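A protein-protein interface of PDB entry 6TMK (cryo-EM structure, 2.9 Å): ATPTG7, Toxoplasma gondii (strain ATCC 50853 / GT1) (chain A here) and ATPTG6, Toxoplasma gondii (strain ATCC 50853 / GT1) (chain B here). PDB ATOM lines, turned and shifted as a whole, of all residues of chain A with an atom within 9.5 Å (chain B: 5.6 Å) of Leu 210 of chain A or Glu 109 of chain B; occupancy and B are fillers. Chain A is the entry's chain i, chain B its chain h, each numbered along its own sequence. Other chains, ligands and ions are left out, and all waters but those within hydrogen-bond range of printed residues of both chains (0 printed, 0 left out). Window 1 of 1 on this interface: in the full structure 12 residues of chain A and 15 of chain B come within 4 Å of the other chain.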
ATOM      1  N   ASP A 198      -2.312  12.929  -3.940  1.00  0.00           N
ATOM      2  CA  ASP A 198      -2.931  12.614  -2.659  1.00  0.00           C
ATOM      3  C   ASP A 198      -1.953  11.896  -1.738  1.00  0.00           C
ATOM      4  O   ASP A 198      -1.960  12.115  -0.523  1.00  0.00           O
ATOM      5  CB  ASP A 198      -4.183  11.771  -2.884  1.00  0.00           C
ATOM      6  CG  ASP A 198      -5.275  12.530  -3.602  1.00  0.00           C
ATOM      7  OD1 ASP A 198      -5.989  11.915  -4.420  1.00  0.00           O
ATOM      8  OD2 ASP A 198      -5.423  13.743  -3.353  1.00  0.00           O
ATOM      9  N   SER A 199      -1.091  11.048  -2.300  1.00  0.00           N
ATOM     10  CA  SER A 199      -0.100  10.362  -1.479  1.00  0.00           C
ATOM     11  C   SER A 199       0.921  11.339  -0.917  1.00  0.00           C
ATOM     12  O   SER A 199       1.297  11.248   0.258  1.00  0.00           O
ATOM     13  CB  SER A 199       0.591   9.273  -2.295  1.00  0.00           C
ATOM     14  OG  SER A 199      -0.298   8.216  -2.585  1.00  0.00           O
ATOM     15  N   PHE A 200       1.383  12.281  -1.740  1.00  0.00           N
ATOM     16  CA  PHE A 200       2.285  13.311  -1.239  1.00  0.00           C
ATOM     17  C   PHE A 200       1.614  14.154  -0.165  1.00  0.00           C
ATOM     18  O   PHE A 200       2.232  14.486   0.850  1.00  0.00           O
ATOM     19  CB  PHE A 200       2.756  14.207  -2.379  1.00  0.00           C
ATOM     20  CG  PHE A 200       3.727  15.255  -1.944  1.00  0.00           C
ATOM     21  CD1 PHE A 200       5.072  14.976  -1.874  1.00  0.00           C
ATOM     22  CD2 PHE A 200       3.292  16.509  -1.573  1.00  0.00           C
ATOM     23  CE1 PHE A 200       5.960  15.927  -1.465  1.00  0.00           C
ATOM     24  CE2 PHE A 200       4.181  17.460  -1.157  1.00  0.00           C
ATOM     25  CZ  PHE A 200       5.515  17.170  -1.102  1.00  0.00           C
ATOM     26  N   PHE A 201       0.360  14.543  -0.392  1.00  0.00           N
ATOM     27  CA  PHE A 201      -0.389  15.291   0.608  1.00  0.00           C
ATOM     28  C   PHE A 201      -0.468  14.535   1.928  1.00  0.00           C
ATOM     29  O   PHE A 201      -0.275  15.115   3.004  1.00  0.00           O
ATOM     30  CB  PHE A 201      -1.787  15.580   0.076  1.00  0.00           C
ATOM     31  CG  PHE A 201      -2.634  16.377   1.005  1.00  0.00           C
ATOM     32  CD1 PHE A 201      -2.370  17.710   1.223  1.00  0.00           C
ATOM     33  CD2 PHE A 201      -3.699  15.796   1.658  1.00  0.00           C
ATOM     34  CE1 PHE A 201      -3.144  18.444   2.072  1.00  0.00           C
ATOM     35  CE2 PHE A 201      -4.475  16.528   2.510  1.00  0.00           C
ATOM     36  CZ  PHE A 201      -4.198  17.855   2.716  1.00  0.00           C
ATOM     37  N   GLN A 202      -0.753  13.238   1.860  1.00  0.00           N
ATOM     38  CA  GLN A 202      -0.879  12.435   3.065  1.00  0.00           C
ATOM     39  C   GLN A 202       0.458  12.361   3.794  1.00  0.00           C
ATOM     40  O   GLN A 202       0.528  12.508   5.021  1.00  0.00           O
ATOM     41  CB  GLN A 202      -1.382  11.049   2.675  1.00  0.00           C
ATOM     42  CG  GLN A 202      -1.877  10.196   3.800  1.00  0.00           C
ATOM     43  CD  GLN A 202      -3.150  10.747   4.396  1.00  0.00           C
ATOM     44  OE1 GLN A 202      -4.087  11.076   3.672  1.00  0.00           O
ATOM     45  NE2 GLN A 202      -3.191  10.866   5.710  1.00  0.00           N
ATOM     46  N   CYS A 203       1.535  12.116   3.045  1.00  0.00           N
ATOM     47  CA  CYS A 203       2.867  12.102   3.638  1.00  0.00           C
ATOM     48  C   CYS A 203       3.206  13.440   4.284  1.00  0.00           C
ATOM     49  O   CYS A 203       3.831  13.485   5.348  1.00  0.00           O
ATOM     50  CB  CYS A 203       3.899  11.756   2.570  1.00  0.00           C
ATOM     51  SG  CYS A 203       3.942  10.033   2.082  1.00  0.00           S
ATOM     52  N   TYR A 204       2.820  14.543   3.643  1.00  0.00           N
ATOM     53  CA  TYR A 204       3.079  15.862   4.203  1.00  0.00           C
ATOM     54  C   TYR A 204       2.323  16.060   5.506  1.00  0.00           C
ATOM     55  O   TYR A 204       2.853  16.636   6.463  1.00  0.00           O
ATOM     56  CB  TYR A 204       2.701  16.934   3.183  1.00  0.00           C
ATOM     57  CG  TYR A 204       2.491  18.300   3.773  1.00  0.00           C
ATOM     58  CD1 TYR A 204       3.523  18.967   4.401  1.00  0.00           C
ATOM     59  CD2 TYR A 204       1.258  18.918   3.713  1.00  0.00           C
ATOM     60  CE1 TYR A 204       3.336  20.207   4.943  1.00  0.00           C
ATOM     61  CE2 TYR A 204       1.063  20.156   4.252  1.00  0.00           C
ATOM     62  CZ  TYR A 204       2.104  20.798   4.872  1.00  0.00           C
ATOM     63  OH  TYR A 204       1.916  22.043   5.415  1.00  0.00           O
ATOM     64  N   ARG A 205       1.078  15.587   5.561  1.00  0.00           N
ATOM     65  CA  ARG A 205       0.319  15.652   6.804  1.00  0.00           C
ATOM     66  C   ARG A 205       0.994  14.852   7.902  1.00  0.00           C
ATOM     67  O   ARG A 205       1.044  15.284   9.059  1.00  0.00           O
ATOM     68  CB  ARG A 205      -1.104  15.146   6.600  1.00  0.00           C
ATOM     69  CG  ARG A 205      -1.959  16.003   5.719  1.00  0.00           C
ATOM     70  CD  ARG A 205      -2.266  17.293   6.428  1.00  0.00           C
ATOM     71  NE  ARG A 205      -3.200  18.142   5.708  1.00  0.00           N
ATOM     72  CZ  ARG A 205      -3.529  19.362   6.112  1.00  0.00           C
ATOM     73  NH1 ARG A 205      -2.976  19.867   7.201  1.00  0.00           N
ATOM     74  NH2 ARG A 205      -4.390  20.082   5.416  1.00  0.00           N
ATOM     75  N   HIS A 206       1.514  13.680   7.564  1.00  0.00           N
ATOM     76  CA  HIS A 206       2.160  12.816   8.536  1.00  0.00           C
ATOM     77  C   HIS A 206       3.662  13.045   8.634  1.00  0.00           C
ATOM     78  O   HIS A 206       4.377  12.191   9.167  1.00  0.00           O
ATOM     79  CB  HIS A 206       1.860  11.360   8.201  1.00  0.00           C
ATOM     80  CG  HIS A 206       0.503  10.921   8.646  1.00  0.00           C
ATOM     81  ND1 HIS A 206      -0.630  11.159   7.903  1.00  0.00           N
ATOM     82  CD2 HIS A 206       0.091  10.298   9.773  1.00  0.00           C
ATOM     83  CE1 HIS A 206      -1.680  10.683   8.544  1.00  0.00           C
ATOM     84  NE2 HIS A 206      -1.269  10.151   9.679  1.00  0.00           N
ATOM     85  N   GLY A 207       4.153  14.175   8.139  1.00  0.00           N
ATOM     86  CA  GLY A 207       5.544  14.532   8.319  1.00  0.00           C
ATOM     87  C   GLY A 207       6.526  13.604   7.654  1.00  0.00           C
ATOM     88  O   GLY A 207       7.683  13.537   8.069  1.00  0.00           O
ATOM     89  N   PHE A 208       6.097  12.876   6.627  1.00  0.00           N
ATOM     90  CA  PHE A 208       6.962  11.946   5.912  1.00  0.00           C
ATOM     91  C   PHE A 208       7.522  10.889   6.856  1.00  0.00           C
ATOM     92  O   PHE A 208       8.681  10.483   6.755  1.00  0.00           O
ATOM     93  CB  PHE A 208       8.080  12.694   5.188  1.00  0.00           C
ATOM     94  CG  PHE A 208       7.583  13.764   4.270  1.00  0.00           C
ATOM     95  CD1 PHE A 208       7.290  13.484   2.953  1.00  0.00           C
ATOM     96  CD2 PHE A 208       7.401  15.050   4.727  1.00  0.00           C
ATOM     97  CE1 PHE A 208       6.825  14.466   2.118  1.00  0.00           C
ATOM     98  CE2 PHE A 208       6.938  16.031   3.894  1.00  0.00           C
ATOM     99  CZ  PHE A 208       6.650  15.739   2.589  1.00  0.00           C
ATOM    100  N   ARG A 209       6.680  10.433   7.778  1.00  0.00           N
ATOM    101  CA  ARG A 209       7.036   9.404   8.740  1.00  0.00           C
ATOM    102  C   ARG A 209       6.646   8.006   8.288  1.00  0.00           C
ATOM    103  O   ARG A 209       7.092   7.030   8.899  1.00  0.00           O
ATOM    104  CB  ARG A 209       6.375   9.692  10.088  1.00  0.00           C
ATOM    105  CG  ARG A 209       6.945  10.872  10.835  1.00  0.00           C
ATOM    106  CD  ARG A 209       6.393  10.953  12.237  1.00  0.00           C
ATOM    107  NE  ARG A 209       4.973  11.281  12.269  1.00  0.00           N
ATOM    108  CZ  ARG A 209       4.489  12.515  12.207  1.00  0.00           C
ATOM    109  NH1 ARG A 209       5.302  13.554  12.114  1.00  0.00           N
ATOM    110  NH2 ARG A 209       3.181  12.709  12.236  1.00  0.00           N
ATOM    111  N   LEU A 210       5.823   7.881   7.255  1.00  0.00           N
ATOM    112  CA  LEU A 210       5.335   6.580   6.845  1.00  0.00           C
ATOM    113  C   LEU A 210       6.360   5.872   5.963  1.00  0.00           C
ATOM    114  O   LEU A 210       7.351   6.455   5.518  1.00  0.00           O
ATOM    115  CB  LEU A 210       4.008   6.718   6.103  1.00  0.00           C
ATOM    116  CG  LEU A 210       3.022   7.752   6.640  1.00  0.00           C
ATOM    117  CD1 LEU A 210       1.881   7.920   5.679  1.00  0.00           C
ATOM    118  CD2 LEU A 210       2.504   7.335   7.995  1.00  0.00           C
ATOM    119  N   GLU A 211       6.102   4.589   5.713  1.00  0.00           N
ATOM    120  CA  GLU A 211       7.016   3.780   4.916  1.00  0.00           C
ATOM    121  C   GLU A 211       7.083   4.276   3.477  1.00  0.00           C
ATOM    122  O   GLU A 211       8.170   4.425   2.909  1.00  0.00           O
ATOM    123  CB  GLU A 211       6.581   2.320   4.959  1.00  0.00           C
ATOM    124  CG  GLU A 211       6.559   1.725   6.359  1.00  0.00           C
ATOM    125  CD  GLU A 211       7.945   1.383   6.875  1.00  0.00           C
ATOM    126  OE1 GLU A 211       8.937   1.725   6.197  1.00  0.00           O
ATOM    127  OE2 GLU A 211       8.041   0.773   7.959  1.00  0.00           O
ATOM    128  N   ALA A 212       5.924   4.538   2.875  1.00  0.00           N
ATOM    129  CA  ALA A 212       5.859   4.985   1.493  1.00  0.00           C
ATOM    130  C   ALA A 212       6.404   6.388   1.300  1.00  0.00           C
ATOM    131  O   ALA A 212       6.651   6.788   0.159  1.00  0.00           O
ATOM    132  CB  ALA A 212       4.418   4.943   1.001  1.00  0.00           C
ATOM    133  N   CYS A 213       6.597   7.138   2.379  1.00  0.00           N
ATOM    134  CA  CYS A 213       7.154   8.475   2.304  1.00  0.00           C
ATOM    135  C   CYS A 213       8.672   8.481   2.381  1.00  0.00           C
ATOM    136  O   CYS A 213       9.287   9.527   2.150  1.00  0.00           O
ATOM    137  CB  CYS A 213       6.583   9.323   3.439  1.00  0.00           C
ATOM    138  SG  CYS A 213       4.803   9.135   3.683  1.00  0.00           S
ATOM    139  N   GLN A 214       9.284   7.347   2.705  1.00  0.00           N
ATOM    140  CA  GLN A 214      10.731   7.273   2.817  1.00  0.00           C
ATOM    141  C   GLN A 214      11.386   7.389   1.447  1.00  0.00           C
ATOM    142  O   GLN A 214      10.892   6.846   0.456  1.00  0.00           O
ATOM    143  CB  GLN A 214      11.140   5.963   3.479  1.00  0.00           C
ATOM    144  CG  GLN A 214      10.724   5.854   4.934  1.00  0.00           C
ATOM    145  CD  GLN A 214      11.511   6.770   5.840  1.00  0.00           C
ATOM    146  OE1 GLN A 214      12.741   6.803   5.797  1.00  0.00           O
ATOM    147  NE2 GLN A 214      10.805   7.526   6.670  1.00  0.00           N
ATOM    148  N   GLY A 215      12.505   8.104   1.399  1.00  0.00           N
ATOM    149  CA  GLY A 215      13.167   8.367   0.138  1.00  0.00           C
ATOM    150  C   GLY A 215      12.588   9.572  -0.583  1.00  0.00           C
ATOM    151  O   GLY A 215      12.108  10.531   0.026  1.00  0.00           O
ATOM    152  N   LYS A 217      10.687   8.864  -3.677  1.00  0.00           N
ATOM    153  CA  LYS A 217       9.729   8.326  -4.632  1.00  0.00           C
ATOM    154  C   LYS A 217       8.403   9.068  -4.572  1.00  0.00           C
ATOM    155  O   LYS A 217       7.757   9.263  -5.606  1.00  0.00           O
ATOM    156  CB  LYS A 217       9.537   6.838  -4.365  1.00  0.00           C
ATOM    157  CG  LYS A 217       8.949   6.547  -3.010  1.00  0.00           C
ATOM    158  CD  LYS A 217       9.035   5.078  -2.682  1.00  0.00           C
ATOM    159  CE  LYS A 217       8.425   4.787  -1.331  1.00  0.00           C
ATOM    160  NZ  LYS A 217       8.686   3.392  -0.904  1.00  0.00           N
ATOM    161  N   ALA A 218       8.008   9.528  -3.385  1.00  0.00           N
ATOM    162  CA  ALA A 218       6.741  10.234  -3.246  1.00  0.00           C
ATOM    163  C   ALA A 218       6.690  11.469  -4.129  1.00  0.00           C
ATOM    164  O   ALA A 218       5.612  11.863  -4.589  1.00  0.00           O
ATOM    165  CB  ALA A 218       6.524  10.621  -1.787  1.00  0.00           C
ATOM    166  N   ARG B  54       5.611  -1.722  15.728  1.00  0.00           N
ATOM    167  CA  ARG B  54       4.880  -0.496  15.987  1.00  0.00           C
ATOM    168  C   ARG B  54       4.680   0.347  14.738  1.00  0.00           C
ATOM    169  O   ARG B  54       3.807   1.219  14.731  1.00  0.00           O
ATOM    170  CB  ARG B  54       5.597   0.333  17.053  1.00  0.00           C
ATOM    171  CG  ARG B  54       5.194  -0.018  18.472  1.00  0.00           C
ATOM    172  CD  ARG B  54       5.368   1.151  19.414  1.00  0.00           C
ATOM    173  NE  ARG B  54       6.762   1.364  19.792  1.00  0.00           N
ATOM    174  CZ  ARG B  54       7.360   2.549  19.835  1.00  0.00           C
ATOM    175  NH1 ARG B  54       6.704   3.658  19.532  1.00  0.00           N
ATOM    176  NH2 ARG B  54       8.629   2.623  20.190  1.00  0.00           N
ATOM    177  N   ARG B  55       5.460   0.103  13.686  1.00  0.00           N
ATOM    178  CA  ARG B  55       5.250   0.802  12.429  1.00  0.00           C
ATOM    179  C   ARG B  55       4.090   0.212  11.651  1.00  0.00           C
ATOM    180  O   ARG B  55       3.391   0.940  10.941  1.00  0.00           O
ATOM    181  CB  ARG B  55       6.514   0.751  11.577  1.00  0.00           C
ATOM    182  CG  ARG B  55       7.518   1.831  11.876  1.00  0.00           C
ATOM    183  CD  ARG B  55       8.420   2.074  10.692  1.00  0.00           C
ATOM    184  NE  ARG B  55       9.151   0.872  10.309  1.00  0.00           N
ATOM    185  CZ  ARG B  55      10.246   0.433  10.918  1.00  0.00           C
ATOM    186  NH1 ARG B  55      10.753   1.101  11.944  1.00  0.00           N
ATOM    187  NH2 ARG B  55      10.837  -0.673  10.495  1.00  0.00           N
ATOM    188  N   SER B 100       1.859  13.475  17.558  1.00  0.00           N
ATOM    189  CA  SER B 100       2.493  12.729  16.478  1.00  0.00           C
ATOM    190  C   SER B 100       3.296  11.552  17.014  1.00  0.00           C
ATOM    191  O   SER B 100       3.201  10.433  16.498  1.00  0.00           O
ATOM    192  CB  SER B 100       3.401  13.657  15.679  1.00  0.00           C
ATOM    193  OG  SER B 100       2.733  14.844  15.302  1.00  0.00           O
ATOM    194  N   VAL B 103       0.883   8.956  19.407  1.00  0.00           N
ATOM    195  CA  VAL B 103      -0.079   8.070  18.765  1.00  0.00           C
ATOM    196  C   VAL B 103       0.574   6.764  18.334  1.00  0.00           C
ATOM    197  O   VAL B 103      -0.097   5.730  18.241  1.00  0.00           O
ATOM    198  CB  VAL B 103      -0.726   8.796  17.574  1.00  0.00           C
ATOM    199  CG1 VAL B 103       0.222   8.842  16.397  1.00  0.00           C
ATOM    200  CG2 VAL B 103      -2.023   8.149  17.201  1.00  0.00           C
ATOM    201  N   SER B 104       1.878   6.787  18.067  1.00  0.00           N
ATOM    202  CA  SER B 104       2.593   5.595  17.634  1.00  0.00           C
ATOM    203  C   SER B 104       2.695   4.543  18.725  1.00  0.00           C
ATOM    204  O   SER B 104       3.017   3.389  18.427  1.00  0.00           O
ATOM    205  CB  SER B 104       3.988   5.985  17.157  1.00  0.00           C
ATOM    206  OG  SER B 104       3.915   6.865  16.054  1.00  0.00           O
ATOM    207  N   PHE B 107      -1.372   3.111  18.164  1.00  0.00           N
ATOM    208  CA  PHE B 107      -1.827   2.797  16.821  1.00  0.00           C
ATOM    209  C   PHE B 107      -0.679   3.010  15.852  1.00  0.00           C
ATOM    210  O   PHE B 107       0.250   3.771  16.138  1.00  0.00           O
ATOM    211  CB  PHE B 107      -3.017   3.664  16.395  1.00  0.00           C
ATOM    212  CG  PHE B 107      -4.071   3.787  17.434  1.00  0.00           C
ATOM    213  CD1 PHE B 107      -5.064   2.844  17.532  1.00  0.00           C
ATOM    214  CD2 PHE B 107      -4.072   4.844  18.312  1.00  0.00           C
ATOM    215  CE1 PHE B 107      -6.032   2.950  18.481  1.00  0.00           C
ATOM    216  CE2 PHE B 107      -5.041   4.953  19.266  1.00  0.00           C
ATOM    217  CZ  PHE B 107      -6.024   4.002  19.352  1.00  0.00           C
ATOM    218  N   PRO B 108      -0.712   2.351  14.697  1.00  0.00           N
ATOM    219  CA  PRO B 108       0.239   2.690  13.640  1.00  0.00           C
ATOM    220  C   PRO B 108      -0.293   3.809  12.760  1.00  0.00           C
ATOM    221  O   PRO B 108      -1.455   3.820  12.348  1.00  0.00           O
ATOM    222  CB  PRO B 108       0.380   1.373  12.865  1.00  0.00           C
ATOM    223  CG  PRO B 108      -0.718   0.485  13.340  1.00  0.00           C
ATOM    224  CD  PRO B 108      -1.564   1.220  14.303  1.00  0.00           C
ATOM    225  N   GLU B 109       0.587   4.768  12.473  1.00  0.00           N
ATOM    226  CA  GLU B 109       0.176   5.970  11.756  1.00  0.00           C
ATOM    227  C   GLU B 109      -0.331   5.644  10.361  1.00  0.00           C
ATOM    228  O   GLU B 109      -1.278   6.272   9.875  1.00  0.00           O
ATOM    229  CB  GLU B 109       1.338   6.951  11.678  1.00  0.00           C
ATOM    230  CG  GLU B 109       1.777   7.507  13.002  1.00  0.00           C
ATOM    231  CD  GLU B 109       2.886   8.530  12.853  1.00  0.00           C
ATOM    232  OE1 GLU B 109       4.007   8.267  13.338  1.00  0.00           O
ATOM    233  OE2 GLU B 109       2.638   9.593  12.245  1.00  0.00           O
ATOM    234  N   GLY B 110       0.281   4.670   9.703  1.00  0.00           N
ATOM    235  CA  GLY B 110      -0.141   4.254   8.391  1.00  0.00           C
ATOM    236  C   GLY B 110      -1.322   3.324   8.368  1.00  0.00           C
ATOM    237  O   GLY B 110      -1.696   2.830   7.302  1.00  0.00           O
ATOM    238  N   GLY B 111      -1.931   3.073   9.518  1.00  0.00           N
ATOM    239  CA  GLY B 111      -3.025   2.136   9.612  1.00  0.00           C
ATOM    240  C   GLY B 111      -2.546   0.706   9.734  1.00  0.00           C
ATOM    241  O   GLY B 111      -1.360   0.391   9.628  1.00  0.00           O
ATOM    242  N   THR B 141      -5.697   5.921   7.295  1.00  0.00           N
ATOM    243  CA  THR B 141      -4.600   6.154   8.213  1.00  0.00           C
ATOM    244  C   THR B 141      -5.148   6.707   9.520  1.00  0.00           C
ATOM    245  O   THR B 141      -6.349   6.928   9.683  1.00  0.00           O
ATOM    246  CB  THR B 141      -3.584   7.128   7.618  1.00  0.00           C
ATOM    247  OG1 THR B 141      -4.255   8.326   7.224  1.00  0.00           O
ATOM    248  CG2 THR B 141      -2.893   6.531   6.421  1.00  0.00           C
ATOM    249  N   THR B 142      -4.249   6.941  10.465  1.00  0.00           N
ATOM    250  CA  THR B 142      -4.616   7.720  11.629  1.00  0.00           C
ATOM    251  C   THR B 142      -4.853   9.171  11.242  1.00  0.00           C
ATOM    252  O   THR B 142      -4.354   9.671  10.232  1.00  0.00           O
ATOM    253  CB  THR B 142      -3.535   7.664  12.705  1.00  0.00           C
ATOM    254  OG1 THR B 142      -2.280   8.062  12.151  1.00  0.00           O
ATOM    255  CG2 THR B 142      -3.422   6.288  13.280  1.00  0.00           C
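NE2 of Gln 202 of chain A is in hydrogen-bond range of OG1 of Thr 141 of chain B (3.1 Å).
The guanidinium group (NE) of Arg 55 of chain B is in salt-bridge range of the side-chain carboxylate (OE2) of Glu 211 of chain A (2.6 Å).
The side-chain carboxylate (OE2) of Glu 109 of chain B is in salt-bridge range of the guanidinium group (NE) of Arg 209 of chain A (2.9 Å).
The backbone carbonyl oxygen of Thr 142 of chain B is in hydrogen-bond range of a ring nitrogen (NE2) of His 206 of chain A, 3.2 Å away.
OG1 of Thr 142 of chain B lies within hydrogen-bond range of O of Glu 109 of chain B, at 3.1 Å.
The side-chain amide nitrogen (NE2) of Gln 202 of chain A sits close to a ring nitrogen (ND1) of His 206 of chain A (3.4 Å).
The backbone carbonyl oxygen (O) of His 206 of chain A lies close to the guanidinium group (NE) of Arg 209 of chain A, at 3.3 Å.
The side-chain sulfur (SG) of Cys 213 of chain A forms a disulfide with the side-chain sulfur (SG) of Cys 203 of chain A, 2.0 Å away.
The side-chain carboxylate (OE1) of Glu 109 of chain B is in hydrogen-bond range of the side-chain hydroxyl (OG) of Ser 104 of chain B (3.1 Å).
Among the printed residues, pairs that only touch across the chains: His 206 of chain A with Glu 109 of chain B, His 206 of chain A with Thr 141 of chain B, Arg 209 of chain A with Ser 100 of chain B, Leu 210 of chain A with Glu 109 of chain B and Leu 210 of chain A with Gly 110 of chain B.
Printed residues of chain B within 4 Å of Gln 202 of chain A: Thr 141 (3.1 Å).
Of the printed residues of chain B, His 206 of chain A touches Glu 109 (3.6 Å), Thr 141 (3.7 Å) and Thr 142 (3.2 Å).
Of the printed residues of chain B, Arg 209 of chain A touches Ser 100 (3.6 Å) and Glu 109 (2.9 Å).
Leu 210 of chain A touches just these residues of chain B: Glu 109 and Gly 110.
Of the printed residues of chain B, Glu 211 of chain A touches Arg 55.
Ala 218 of chain A touches none of the printed residues of chain B.
Arg 54 of chain B touches none of the printed residues of chain A.
No residue of chain A comes within 4 Å of Pro 108 of chain B.
Of chain A, only His 206, Arg 209 and Leu 210 come within 4 Å of Glu 109 of chain B.
No residue of chain A comes within 4 Å of Gly 111 of chain B.
Thr 141 of chain B touches just these residues of chain A: Gln 202 and His 206.
Of chain A, only His 206 comes within 4 Å of Thr 142 of chain B.
The nearest residue of chain B that does not touch Leu 210 of chain A is Thr 141 of chain B (5.0 Å).
The nearest printed residue of chain B that does not touch Arg 209 of chain A is Arg 55 of chain B (5.4 Å).
Hydrophobic or aromatic side chains of chain A that line the printed part of chain B: His 206 and Leu 210.
Printed residues of chain B that touch a printed residue of chain A: Arg 55, Ser 100, Glu 109, Gly 110, Thr 141 and Thr 142.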
